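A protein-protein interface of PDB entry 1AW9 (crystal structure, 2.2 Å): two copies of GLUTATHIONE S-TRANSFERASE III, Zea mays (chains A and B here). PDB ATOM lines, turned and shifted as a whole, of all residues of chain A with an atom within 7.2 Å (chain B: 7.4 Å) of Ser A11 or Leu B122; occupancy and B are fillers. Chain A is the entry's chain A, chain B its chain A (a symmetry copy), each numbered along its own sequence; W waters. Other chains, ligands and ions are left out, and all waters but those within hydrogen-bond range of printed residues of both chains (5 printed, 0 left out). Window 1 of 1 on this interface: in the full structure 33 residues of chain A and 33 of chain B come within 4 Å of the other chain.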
ATOM      1  N   GLY A   7     -22.363  16.882  -0.615  1.00  0.00           N
ATOM      2  CA  GLY A   7     -20.948  16.765  -0.864  1.00  0.00           C
ATOM      3  C   GLY A   7     -20.566  15.430  -1.426  1.00  0.00           C
ATOM      4  O   GLY A   7     -21.375  14.523  -1.538  1.00  0.00           O
ATOM      5  N   MET A   8     -19.306  15.328  -1.803  1.00  0.00           N
ATOM      6  CA  MET A   8     -18.747  14.106  -2.356  1.00  0.00           C
ATOM      7  C   MET A   8     -18.435  13.170  -1.205  1.00  0.00           C
ATOM      8  O   MET A   8     -17.787  13.579  -0.238  1.00  0.00           O
ATOM      9  CB  MET A   8     -17.416  14.425  -3.017  1.00  0.00           C
ATOM     10  CG  MET A   8     -17.376  14.409  -4.520  1.00  0.00           C
ATOM     11  SD  MET A   8     -15.618  14.556  -4.933  1.00  0.00           S
ATOM     12  CE  MET A   8     -15.108  12.737  -5.393  1.00  0.00           C
ATOM     13  N   PRO A   9     -18.858  11.898  -1.293  1.00  0.00           N
ATOM     14  CA  PRO A   9     -18.565  10.959  -0.194  1.00  0.00           C
ATOM     15  C   PRO A   9     -17.066  10.687   0.073  1.00  0.00           C
ATOM     16  O   PRO A   9     -16.710  10.165   1.126  1.00  0.00           O
ATOM     17  CB  PRO A   9     -19.337   9.689  -0.594  1.00  0.00           C
ATOM     18  CG  PRO A   9     -19.608   9.857  -2.068  1.00  0.00           C
ATOM     19  CD  PRO A   9     -19.865  11.333  -2.213  1.00  0.00           C
ATOM     20  N   LEU A  10     -16.193  11.082  -0.854  1.00  0.00           N
ATOM     21  CA  LEU A  10     -14.756  10.860  -0.679  1.00  0.00           C
ATOM     22  C   LEU A  10     -14.030  11.987   0.030  1.00  0.00           C
ATOM     23  O   LEU A  10     -12.924  11.795   0.521  1.00  0.00           O
ATOM     24  CB  LEU A  10     -14.081  10.594  -2.017  1.00  0.00           C
ATOM     25  CG  LEU A  10     -14.370   9.174  -2.495  1.00  0.00           C
ATOM     26  CD1 LEU A  10     -13.866   8.988  -3.915  1.00  0.00           C
ATOM     27  CD2 LEU A  10     -13.743   8.164  -1.542  1.00  0.00           C
ATOM     28  N   SER A  11     -14.630  13.166   0.037  1.00  0.00           N
ATOM     29  CA  SER A  11     -14.033  14.313   0.668  1.00  0.00           C
ATOM     30  C   SER A  11     -13.959  14.149   2.194  1.00  0.00           C
ATOM     31  O   SER A  11     -14.998  14.064   2.877  1.00  0.00           O
ATOM     32  CB  SER A  11     -14.835  15.541   0.288  1.00  0.00           C
ATOM     33  OG  SER A  11     -14.938  16.425   1.384  1.00  0.00           O
ATOM     34  N   PRO A  12     -12.733  14.190   2.764  1.00  0.00           N
ATOM     35  CA  PRO A  12     -12.576  14.033   4.212  1.00  0.00           C
ATOM     36  C   PRO A  12     -13.364  15.053   5.034  1.00  0.00           C
ATOM     37  O   PRO A  12     -13.635  14.843   6.221  1.00  0.00           O
ATOM     38  CB  PRO A  12     -11.058  14.204   4.427  1.00  0.00           C
ATOM     39  CG  PRO A  12     -10.448  13.799   3.138  1.00  0.00           C
ATOM     40  CD  PRO A  12     -11.426  14.398   2.115  1.00  0.00           C
ATOM     41  N   ASN A  13     -13.706  16.174   4.425  1.00  0.00           N
ATOM     42  CA  ASN A  13     -14.432  17.179   5.161  1.00  0.00           C
ATOM     43  C   ASN A  13     -15.889  16.752   5.249  1.00  0.00           C
ATOM     44  O   ASN A  13     -16.577  17.089   6.212  1.00  0.00           O
ATOM     45  CB  ASN A  13     -14.217  18.564   4.548  1.00  0.00           C
ATOM     46  CG  ASN A  13     -12.835  19.150   4.890  1.00  0.00           C
ATOM     47  OD1 ASN A  13     -12.365  19.026   6.016  1.00  0.00           O
ATOM     48  ND2 ASN A  13     -12.170  19.750   3.910  1.00  0.00           N
ATOM     49  N   VAL A  14     -16.348  15.968   4.270  1.00  0.00           N
ATOM     50  CA  VAL A  14     -17.717  15.435   4.303  1.00  0.00           C
ATOM     51  C   VAL A  14     -17.683  14.283   5.299  1.00  0.00           C
ATOM     52  O   VAL A  14     -18.537  14.182   6.168  1.00  0.00           O
ATOM     53  CB  VAL A  14     -18.183  14.920   2.934  1.00  0.00           C
ATOM     54  CG1 VAL A  14     -19.481  14.090   3.053  1.00  0.00           C
ATOM     55  CG2 VAL A  14     -18.405  16.096   2.033  1.00  0.00           C
ATOM     56  N   VAL A  15     -16.634  13.464   5.244  1.00  0.00           N
ATOM     57  CA  VAL A  15     -16.504  12.357   6.184  1.00  0.00           C
ATOM     58  C   VAL A  15     -16.425  12.824   7.649  1.00  0.00           C
ATOM     59  O   VAL A  15     -16.860  12.104   8.536  1.00  0.00           O
ATOM     60  CB  VAL A  15     -15.324  11.444   5.818  1.00  0.00           C
ATOM     61  CG1 VAL A  15     -15.167  10.302   6.851  1.00  0.00           C
ATOM     62  CG2 VAL A  15     -15.528  10.893   4.424  1.00  0.00           C
ATOM     63  N   ARG A  16     -15.890  14.017   7.916  1.00  0.00           N
ATOM     64  CA  ARG A  16     -15.824  14.518   9.284  1.00  0.00           C
ATOM     65  C   ARG A  16     -17.231  14.724   9.843  1.00  0.00           C
ATOM     66  O   ARG A  16     -17.440  14.678  11.070  1.00  0.00           O
ATOM     67  CB  ARG A  16     -15.088  15.869   9.369  1.00  0.00           C
ATOM     68  CG  ARG A  16     -14.967  16.448  10.824  1.00  0.00           C
ATOM     69  CD  ARG A  16     -14.405  17.915  10.994  1.00  0.00           C
ATOM     70  NE  ARG A  16     -12.990  18.006  10.630  1.00  0.00           N
ATOM     71  CZ  ARG A  16     -12.556  18.445   9.450  1.00  0.00           C
ATOM     72  NH1 ARG A  16     -13.425  18.880   8.541  1.00  0.00           N
ATOM     73  NH2 ARG A  16     -11.294  18.233   9.089  1.00  0.00           N
ATOM     74  N   VAL A  17     -18.167  15.087   8.964  1.00  0.00           N
ATOM     75  CA  VAL A  17     -19.551  15.338   9.393  1.00  0.00           C
ATOM     76  C   VAL A  17     -20.281  14.015   9.550  1.00  0.00           C
ATOM     77  O   VAL A  17     -20.953  13.808  10.541  1.00  0.00           O
ATOM     78  CB  VAL A  17     -20.319  16.263   8.429  1.00  0.00           C
ATOM     79  CG1 VAL A  17     -21.729  16.497   8.949  1.00  0.00           C
ATOM     80  CG2 VAL A  17     -19.597  17.589   8.315  1.00  0.00           C
ATOM     81  N   VAL A  33     -23.226  17.087  -5.187  1.00  0.00           N
ATOM     82  CA  VAL A  33     -23.705  18.250  -5.922  1.00  0.00           C
ATOM     83  C   VAL A  33     -22.738  18.849  -6.910  1.00  0.00           C
ATOM     84  O   VAL A  33     -21.519  18.743  -6.776  1.00  0.00           O
ATOM     85  CB  VAL A  33     -24.183  19.407  -4.990  1.00  0.00           C
ATOM     86  CG1 VAL A  33     -25.613  19.156  -4.544  1.00  0.00           C
ATOM     87  CG2 VAL A  33     -23.239  19.587  -3.785  1.00  0.00           C
ATOM     88  N   ASP A  34     -23.318  19.446  -7.939  1.00  0.00           N
ATOM     89  CA  ASP A  34     -22.576  20.121  -8.984  1.00  0.00           C
ATOM     90  C   ASP A  34     -22.400  21.532  -8.452  1.00  0.00           C
ATOM     91  O   ASP A  34     -23.376  22.272  -8.315  1.00  0.00           O
ATOM     92  CB  ASP A  34     -23.405  20.149 -10.270  1.00  0.00           C
ATOM     93  CG  ASP A  34     -22.597  20.573 -11.486  1.00  0.00           C
ATOM     94  OD1 ASP A  34     -22.348  21.788 -11.643  1.00  0.00           O
ATOM     95  OD2 ASP A  34     -22.236  19.688 -12.295  1.00  0.00           O
ATOM     96  N   LEU A  35     -21.162  21.873  -8.101  1.00  0.00           N
ATOM     97  CA  LEU A  35     -20.833  23.197  -7.558  1.00  0.00           C
ATOM     98  C   LEU A  35     -20.928  24.295  -8.610  1.00  0.00           C
ATOM     99  O   LEU A  35     -21.597  25.322  -8.420  1.00  0.00           O
ATOM    100  CB  LEU A  35     -19.427  23.182  -6.958  1.00  0.00           C
ATOM    101  CG  LEU A  35     -19.376  23.250  -5.445  1.00  0.00           C
ATOM    102  CD1 LEU A  35     -20.396  22.305  -4.840  1.00  0.00           C
ATOM    103  CD2 LEU A  35     -17.985  22.904  -5.006  1.00  0.00           C
ATOM    104  N   THR A  36     -20.220  24.079  -9.709  1.00  0.00           N
ATOM    105  CA  THR A  36     -20.193  25.014 -10.819  1.00  0.00           C
ATOM    106  C   THR A  36     -20.020  24.218 -12.107  1.00  0.00           C
ATOM    107  O   THR A  36     -20.268  24.732 -13.196  1.00  0.00           O
ATOM    108  CB  THR A  36     -19.002  26.006 -10.676  1.00  0.00           C
ATOM    109  OG1 THR A  36     -17.765  25.278 -10.590  1.00  0.00           O
ATOM    110  CG2 THR A  36     -19.166  26.906  -9.423  1.00  0.00           C
ATOM    111  N   THR A  37     -19.709  22.929 -11.944  1.00  0.00           N
ATOM    112  CA  THR A  37     -19.448  21.978 -13.030  1.00  0.00           C
ATOM    113  C   THR A  37     -20.541  21.846 -14.091  1.00  0.00           C
ATOM    114  O   THR A  37     -20.577  20.870 -14.817  1.00  0.00           O
ATOM    115  CB  THR A  37     -19.060  20.541 -12.464  1.00  0.00           C
ATOM    116  OG1 THR A  37     -18.445  20.655 -11.161  1.00  0.00           O
ATOM    117  CG2 THR A  37     -18.069  19.837 -13.400  1.00  0.00           C
ATOM    118  N   GLY A  52     -19.798  28.809  -1.307  1.00  0.00           N
ATOM    119  CA  GLY A  52     -19.679  27.795  -2.342  1.00  0.00           C
ATOM    120  C   GLY A  52     -18.777  26.615  -2.048  1.00  0.00           C
ATOM    121  O   GLY A  52     -18.185  26.050  -2.977  1.00  0.00           O
ATOM    122  N   GLN A  53     -18.656  26.266  -0.769  1.00  0.00           N
ATOM    123  CA  GLN A  53     -17.845  25.135  -0.337  1.00  0.00           C
ATOM    124  C   GLN A  53     -18.721  24.043   0.258  1.00  0.00           C
ATOM    125  O   GLN A  53     -19.829  24.275   0.772  1.00  0.00           O
ATOM    126  CB  GLN A  53     -16.786  25.553   0.699  1.00  0.00           C
ATOM    127  CG  GLN A  53     -15.544  26.173   0.096  1.00  0.00           C
ATOM    128  CD  GLN A  53     -15.051  27.378   0.892  1.00  0.00           C
ATOM    129  OE1 GLN A  53     -14.847  27.289   2.105  1.00  0.00           O
ATOM    130  NE2 GLN A  53     -14.879  28.520   0.214  1.00  0.00           N
ATOM    131  N   ILE A  54     -18.210  22.838   0.104  1.00  0.00           N
ATOM    132  CA  ILE A  54     -18.803  21.605   0.590  1.00  0.00           C
ATOM    133  C   ILE A  54     -18.109  21.334   1.951  1.00  0.00           C
ATOM    134  O   ILE A  54     -16.915  21.641   2.110  1.00  0.00           O
ATOM    135  CB  ILE A  54     -18.503  20.504  -0.475  1.00  0.00           C
ATOM    136  CG1 ILE A  54     -19.488  20.634  -1.628  1.00  0.00           C
ATOM    137  CG2 ILE A  54     -18.419  19.132   0.117  1.00  0.00           C
ATOM    138  CD1 ILE A  54     -20.901  20.821  -1.187  1.00  0.00           C
ATOM    139  N   PRO A  55     -18.818  20.736   2.933  1.00  0.00           N
ATOM    140  CA  PRO A  55     -20.210  20.302   2.856  1.00  0.00           C
ATOM    141  C   PRO A  55     -21.201  21.333   3.362  1.00  0.00           C
ATOM    142  O   PRO A  55     -20.831  22.392   3.877  1.00  0.00           O
ATOM    143  CB  PRO A  55     -20.212  19.094   3.786  1.00  0.00           C
ATOM    144  CG  PRO A  55     -19.352  19.577   4.909  1.00  0.00           C
ATOM    145  CD  PRO A  55     -18.193  20.234   4.178  1.00  0.00           C
ATOM    146  N   SER A 170     -11.557  11.601  10.354  1.00  0.00           N
ATOM    147  CA  SER A 170     -11.457  11.474   8.901  1.00  0.00           C
ATOM    148  C   SER A 170     -10.071  11.774   8.402  1.00  0.00           C
ATOM    149  O   SER A 170      -9.567  11.058   7.548  1.00  0.00           O
ATOM    150  CB  SER A 170     -12.496  12.302   8.158  1.00  0.00           C
ATOM    151  OG  SER A 170     -12.310  13.670   8.340  1.00  0.00           O
ATOM    152  N   TYR A 171      -9.430  12.798   8.949  1.00  0.00           N
ATOM    153  CA  TYR A 171      -8.088  13.113   8.522  1.00  0.00           C
ATOM    154  C   TYR A 171      -7.039  12.133   9.020  1.00  0.00           C
ATOM    155  O   TYR A 171      -6.077  11.872   8.300  1.00  0.00           O
ATOM    156  CB  TYR A 171      -7.744  14.568   8.770  1.00  0.00           C
ATOM    157  CG  TYR A 171      -8.132  15.428   7.572  1.00  0.00           C
ATOM    158  CD1 TYR A 171      -7.271  15.566   6.481  1.00  0.00           C
ATOM    159  CD2 TYR A 171      -9.369  16.087   7.517  1.00  0.00           C
ATOM    160  CE1 TYR A 171      -7.623  16.331   5.378  1.00  0.00           C
ATOM    161  CE2 TYR A 171      -9.731  16.864   6.400  1.00  0.00           C
ATOM    162  CZ  TYR A 171      -8.845  16.975   5.345  1.00  0.00           C
ATOM    163  OH  TYR A 171      -9.165  17.757   4.252  1.00  0.00           O
ATOM    164  N   TYR A 174      -7.369   9.265   6.473  1.00  0.00           N
ATOM    165  CA  TYR A 174      -6.687   9.530   5.205  1.00  0.00           C
ATOM    166  C   TYR A 174      -5.169   9.577   5.345  1.00  0.00           C
ATOM    167  O   TYR A 174      -4.465   9.054   4.490  1.00  0.00           O
ATOM    168  CB  TYR A 174      -7.235  10.798   4.553  1.00  0.00           C
ATOM    169  CG  TYR A 174      -8.569  10.565   3.890  1.00  0.00           C
ATOM    170  CD1 TYR A 174      -9.702  10.285   4.646  1.00  0.00           C
ATOM    171  CD2 TYR A 174      -8.698  10.592   2.501  1.00  0.00           C
ATOM    172  CE1 TYR A 174     -10.940  10.035   4.037  1.00  0.00           C
ATOM    173  CE2 TYR A 174      -9.928  10.348   1.884  1.00  0.00           C
ATOM    174  CZ  TYR A 174     -11.047  10.074   2.656  1.00  0.00           C
ATOM    175  OH  TYR A 174     -12.278   9.893   2.065  1.00  0.00           O
ATOM    176  N   ILE A 210     -17.404   5.086   2.727  1.00  0.00           N
ATOM    177  CA  ILE A 210     -16.524   5.766   1.776  1.00  0.00           C
ATOM    178  C   ILE A 210     -16.354   4.882   0.545  1.00  0.00           C
ATOM    179  O   ILE A 210     -15.863   3.748   0.649  1.00  0.00           O
ATOM    180  CB  ILE A 210     -15.133   6.051   2.369  1.00  0.00           C
ATOM    181  CG1 ILE A 210     -15.245   6.828   3.686  1.00  0.00           C
ATOM    182  CG2 ILE A 210     -14.316   6.872   1.382  1.00  0.00           C
ATOM    183  CD1 ILE A 210     -13.949   6.853   4.485  1.00  0.00           C
ATOM    184  N   PRO A 211     -16.722   5.407  -0.644  1.00  0.00           N
ATOM    185  CA  PRO A 211     -16.649   4.731  -1.951  1.00  0.00           C
ATOM    186  C   PRO A 211     -15.208   4.596  -2.432  1.00  0.00           C
ATOM    187  O   PRO A 211     -14.881   5.035  -3.546  1.00  0.00           O
ATOM    188  CB  PRO A 211     -17.434   5.675  -2.857  1.00  0.00           C
ATOM    189  CG  PRO A 211     -17.061   6.985  -2.327  1.00  0.00           C
ATOM    190  CD  PRO A 211     -17.151   6.803  -0.822  1.00  0.00           C
ATOM    191  N   LEU B  10     -13.504  11.204 -13.736  1.00  0.00           N
ATOM    192  CA  LEU B  10     -13.655  12.657 -13.631  1.00  0.00           C
ATOM    193  C   LEU B  10     -12.386  13.440 -13.905  1.00  0.00           C
ATOM    194  O   LEU B  10     -12.443  14.636 -14.168  1.00  0.00           O
ATOM    195  CB  LEU B  10     -14.199  13.048 -12.265  1.00  0.00           C
ATOM    196  CG  LEU B  10     -15.695  12.760 -12.175  1.00  0.00           C
ATOM    197  CD1 LEU B  10     -16.182  12.962 -10.751  1.00  0.00           C
ATOM    198  CD2 LEU B  10     -16.456  13.641 -13.157  1.00  0.00           C
ATOM    199  N   PHE B 115      -8.093  23.189 -11.159  1.00  0.00           N
ATOM    200  CA  PHE B 115      -7.858  22.709  -9.829  1.00  0.00           C
ATOM    201  C   PHE B 115      -8.358  23.632  -8.711  1.00  0.00           C
ATOM    202  O   PHE B 115      -8.945  23.172  -7.732  1.00  0.00           O
ATOM    203  CB  PHE B 115      -6.396  22.442  -9.592  1.00  0.00           C
ATOM    204  CG  PHE B 115      -6.121  22.164  -8.183  1.00  0.00           C
ATOM    205  CD1 PHE B 115      -6.608  20.998  -7.606  1.00  0.00           C
ATOM    206  CD2 PHE B 115      -5.535  23.135  -7.374  1.00  0.00           C
ATOM    207  CE1 PHE B 115      -6.532  20.795  -6.247  1.00  0.00           C
ATOM    208  CE2 PHE B 115      -5.452  22.942  -6.011  1.00  0.00           C
ATOM    209  CZ  PHE B 115      -5.957  21.767  -5.443  1.00  0.00           C
ATOM    210  N   GLN B 116      -8.020  24.911  -8.788  1.00  0.00           N
ATOM    211  CA  GLN B 116      -8.448  25.869  -7.782  1.00  0.00           C
ATOM    212  C   GLN B 116      -9.953  26.187  -7.822  1.00  0.00           C
ATOM    213  O   GLN B 116     -10.586  26.364  -6.782  1.00  0.00           O
ATOM    214  CB  GLN B 116      -7.672  27.175  -7.949  1.00  0.00           C
ATOM    215  CG  GLN B 116      -6.216  27.076  -7.707  1.00  0.00           C
ATOM    216  CD  GLN B 116      -5.918  26.838  -6.277  1.00  0.00           C
ATOM    217  OE1 GLN B 116      -6.673  27.252  -5.401  1.00  0.00           O
ATOM    218  NE2 GLN B 116      -4.830  26.166  -6.008  1.00  0.00           N
ATOM    219  N   LEU B 117     -10.518  26.287  -9.021  1.00  0.00           N
ATOM    220  CA  LEU B 117     -11.913  26.677  -9.161  1.00  0.00           C
ATOM    221  C   LEU B 117     -12.943  25.552  -9.147  1.00  0.00           C
ATOM    222  O   LEU B 117     -14.113  25.817  -8.882  1.00  0.00           O
ATOM    223  CB  LEU B 117     -12.093  27.538 -10.432  1.00  0.00           C
ATOM    224  CG  LEU B 117     -11.218  28.785 -10.572  1.00  0.00           C
ATOM    225  CD1 LEU B 117     -11.232  29.317 -12.001  1.00  0.00           C
ATOM    226  CD2 LEU B 117     -11.700  29.832  -9.600  1.00  0.00           C
ATOM    227  N   LEU B 118     -12.521  24.316  -9.436  1.00  0.00           N
ATOM    228  CA  LEU B 118     -13.428  23.161  -9.456  1.00  0.00           C
ATOM    229  C   LEU B 118     -13.185  22.100  -8.399  1.00  0.00           C
ATOM    230  O   LEU B 118     -14.121  21.687  -7.718  1.00  0.00           O
ATOM    231  CB  LEU B 118     -13.391  22.473 -10.804  1.00  0.00           C
ATOM    232  CG  LEU B 118     -14.160  23.171 -11.904  1.00  0.00           C
ATOM    233  CD1 LEU B 118     -14.027  22.351 -13.165  1.00  0.00           C
ATOM    234  CD2 LEU B 118     -15.614  23.299 -11.504  1.00  0.00           C
ATOM    235  N   VAL B 119     -11.938  21.644  -8.296  1.00  0.00           N
ATOM    236  CA  VAL B 119     -11.549  20.600  -7.352  1.00  0.00           C
ATOM    237  C   VAL B 119     -11.546  21.016  -5.874  1.00  0.00           C
ATOM    238  O   VAL B 119     -12.182  20.374  -5.039  1.00  0.00           O
ATOM    239  CB  VAL B 119     -10.160  20.063  -7.715  1.00  0.00           C
ATOM    240  CG1 VAL B 119      -9.735  18.922  -6.752  1.00  0.00           C
ATOM    241  CG2 VAL B 119     -10.144  19.615  -9.192  1.00  0.00           C
ATOM    242  N   ARG B 120     -10.807  22.074  -5.550  1.00  0.00           N
ATOM    243  CA  ARG B 120     -10.718  22.554  -4.181  1.00  0.00           C
ATOM    244  C   ARG B 120     -12.029  22.806  -3.485  1.00  0.00           C
ATOM    245  O   ARG B 120     -12.183  22.426  -2.340  1.00  0.00           O
ATOM    246  CB  ARG B 120      -9.834  23.789  -4.075  1.00  0.00           C
ATOM    247  CG  ARG B 120      -8.413  23.453  -4.358  1.00  0.00           C
ATOM    248  CD  ARG B 120      -7.504  24.504  -3.855  1.00  0.00           C
ATOM    249  NE  ARG B 120      -7.561  24.566  -2.406  1.00  0.00           N
ATOM    250  CZ  ARG B 120      -7.171  25.619  -1.697  1.00  0.00           C
ATOM    251  NH1 ARG B 120      -6.685  26.702  -2.312  1.00  0.00           N
ATOM    252  NH2 ARG B 120      -7.291  25.601  -0.371  1.00  0.00           N
ATOM    253  N   PRO B 121     -12.953  23.534  -4.130  1.00  0.00           N
ATOM    254  CA  PRO B 121     -14.223  23.775  -3.462  1.00  0.00           C
ATOM    255  C   PRO B 121     -14.935  22.434  -3.216  1.00  0.00           C
ATOM    256  O   PRO B 121     -15.583  22.267  -2.201  1.00  0.00           O
ATOM    257  CB  PRO B 121     -14.967  24.649  -4.471  1.00  0.00           C
ATOM    258  CG  PRO B 121     -13.881  25.346  -5.185  1.00  0.00           C
ATOM    259  CD  PRO B 121     -12.899  24.255  -5.414  1.00  0.00           C
ATOM    260  N   LEU B 122     -14.802  21.471  -4.119  1.00  0.00           N
ATOM    261  CA  LEU B 122     -15.436  20.167  -3.909  1.00  0.00           C
ATOM    262  C   LEU B 122     -14.845  19.451  -2.687  1.00  0.00           C
ATOM    263  O   LEU B 122     -15.462  18.570  -2.103  1.00  0.00           O
ATOM    264  CB  LEU B 122     -15.266  19.276  -5.137  1.00  0.00           C
ATOM    265  CG  LEU B 122     -16.095  19.588  -6.382  1.00  0.00           C
ATOM    266  CD1 LEU B 122     -15.658  18.693  -7.532  1.00  0.00           C
ATOM    267  CD2 LEU B 122     -17.581  19.402  -6.105  1.00  0.00           C
ATOM    268  N   LEU B 123     -13.650  19.858  -2.308  1.00  0.00           N
ATOM    269  CA  LEU B 123     -12.960  19.286  -1.172  1.00  0.00           C
ATOM    270  C   LEU B 123     -12.995  20.185   0.067  1.00  0.00           C
ATOM    271  O   LEU B 123     -12.184  20.027   0.979  1.00  0.00           O
ATOM    272  CB  LEU B 123     -11.495  19.060  -1.550  1.00  0.00           C
ATOM    273  CG  LEU B 123     -11.023  17.741  -2.146  1.00  0.00           C
ATOM    274  CD1 LEU B 123     -12.131  17.010  -2.901  1.00  0.00           C
ATOM    275  CD2 LEU B 123      -9.832  18.084  -3.038  1.00  0.00           C
ATOM    276  N   GLY B 124     -13.856  21.184   0.080  1.00  0.00           N
ATOM    277  CA  GLY B 124     -13.908  22.042   1.250  1.00  0.00           C
ATOM    278  C   GLY B 124     -12.915  23.183   1.297  1.00  0.00           C
ATOM    279  O   GLY B 124     -12.759  23.809   2.339  1.00  0.00           O
ATOM    280  N   GLY B 125     -12.268  23.508   0.185  1.00  0.00           N
ATOM    281  CA  GLY B 125     -11.327  24.621   0.195  1.00  0.00           C
ATOM    282  C   GLY B 125     -11.679  25.775  -0.736  1.00  0.00           C
ATOM    283  O   GLY B 125     -12.348  25.599  -1.762  1.00  0.00           O
ATOM    284  N   PRO B 213     -21.802  15.221 -11.450  1.00  0.00           N
ATOM    285  CA  PRO B 213     -22.923  15.294 -10.518  1.00  0.00           C
ATOM    286  C   PRO B 213     -24.066  16.178 -10.992  1.00  0.00           C
ATOM    287  O   PRO B 213     -23.936  16.964 -11.945  1.00  0.00           O
ATOM    288  CB  PRO B 213     -22.269  15.821  -9.243  1.00  0.00           C
ATOM    289  CG  PRO B 213     -21.161  16.726  -9.772  1.00  0.00           C
ATOM    290  CD  PRO B 213     -20.599  15.889 -10.897  1.00  0.00           C
HETATM  291  O   HOH W   1     -12.137  17.229   2.145  1.00  0.00           O
HETATM  292  O   HOH W   2     -15.356  19.051   1.454  1.00  0.00           O
HETATM  293  O   HOH W   3     -14.722  22.560   4.223  1.00  0.00           O
HETATM  294  O   HOH W   4     -17.039  22.090  -8.492  1.00  0.00           O
HETATM  295  O   HOH W   5     -16.847  24.773  -7.932  1.00  0.00           O
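ND2 of Asn A13 lies within hydrogen-bond range of O of Leu B123. The side-chain carboxylate (OD2) of Asp A34 sits close to the backbone carbonyl oxygen (O) of Pro B213, at 3.2 Å.
OD1 of Asp A34 is in hydrogen-bond range of N of Thr A37. The side-chain hydroxyl of Ser A11 is in hydrogen-bond range of the backbone NH of Val A14, 3.2 Å away. OG of Ser A11 sits close to N of Asn A13 (3.3 Å). OD1 of Asn A13 lies within hydrogen-bond range of NH1 of Arg A16 (2.7 Å). The backbone carbonyl oxygen of Arg B120 sits at hydrogen-bond distance from the backbone NH of Gly B125, 2.7 Å away.
Leu B122 touches Ser A11 (O to CB, 3.9 Å). Asn A13 touches Gly B124. Pro B213 touches Val A33 (CG to O, 3.6 Å). Pro B121 touches Leu A35 (CB to CD2, 3.5 Å). Leu A35 touches Leu B122. Leu B118 touches Thr A36. Thr A37 touches Leu B118. CG of Gln A53 touches O of Gly B125, at 3.7 Å. N of Ile A54 touches O of Pro B121, 3.5 Å away. Ile A54 touches Gly B124.
Of chain B, only Leu B122 (3.9 Å) comes within 4 Å of Ser A11. Printed residues of chain B within 4 Å of Asn A13: Leu B123 (2.9 Å) and Gly B124 (3.9 Å). Of the printed residues of chain B, Thr A36 touches Leu B118 (3.1 Å). Of the printed residues of chain B, Gln A53 touches Gly B125 (3.7 Å). Of chain A, only Ser A11, Leu A35 and Ile A54 come within 4 Å of Leu B122. Printed residues of chain A within 4 Å of Leu B123: Asn A13 (2.9 Å). The nearest printed residue of chain A that does not touch Leu B123 is Ser A11 (4.3 Å).
Of the 13 printed residues of chain B, 7 touch a printed residue of chain A. Hydrophobic or aromatic side chains of chain B within 4 Å of the printed part of chain A: Leu B118, Pro B121, Leu B122 and Pro B213. Printed residues of chain A that touch a printed residue of chain B: Ser A11, Asn A13, Val A33, Asp A34, Leu A35, Thr A36, Thr A37, Gly A52, Gln A53 and Ile A54. Among the printed residues, 14 pairs touch across the chains.
Position printed for both chains: 10.
Water W2 lies within hydrogen-bond range of the side-chain hydroxyl of Ser A11, the backbone NH of Gly B124, the backbone carbonyl oxygen of Ile A54 and the backbone carbonyl oxygen of Leu B123. Water W5 bridges OG1 of Thr A36 (2.9 Å) and O of Leu B117 (3.1 Å). Water W1 lies within hydrogen-bond range of N of Asn A13 (3.0 Å), OG of Ser A11 (3.0 Å) and O of Leu B123 (3.0 Å). Water W3 lies within hydrogen-bond range of O of Gly B124 and O of Ile A54. Water W4 bridges O of Leu B118 (3.0 Å) and OG1 of Thr A37 (3.3 Å).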
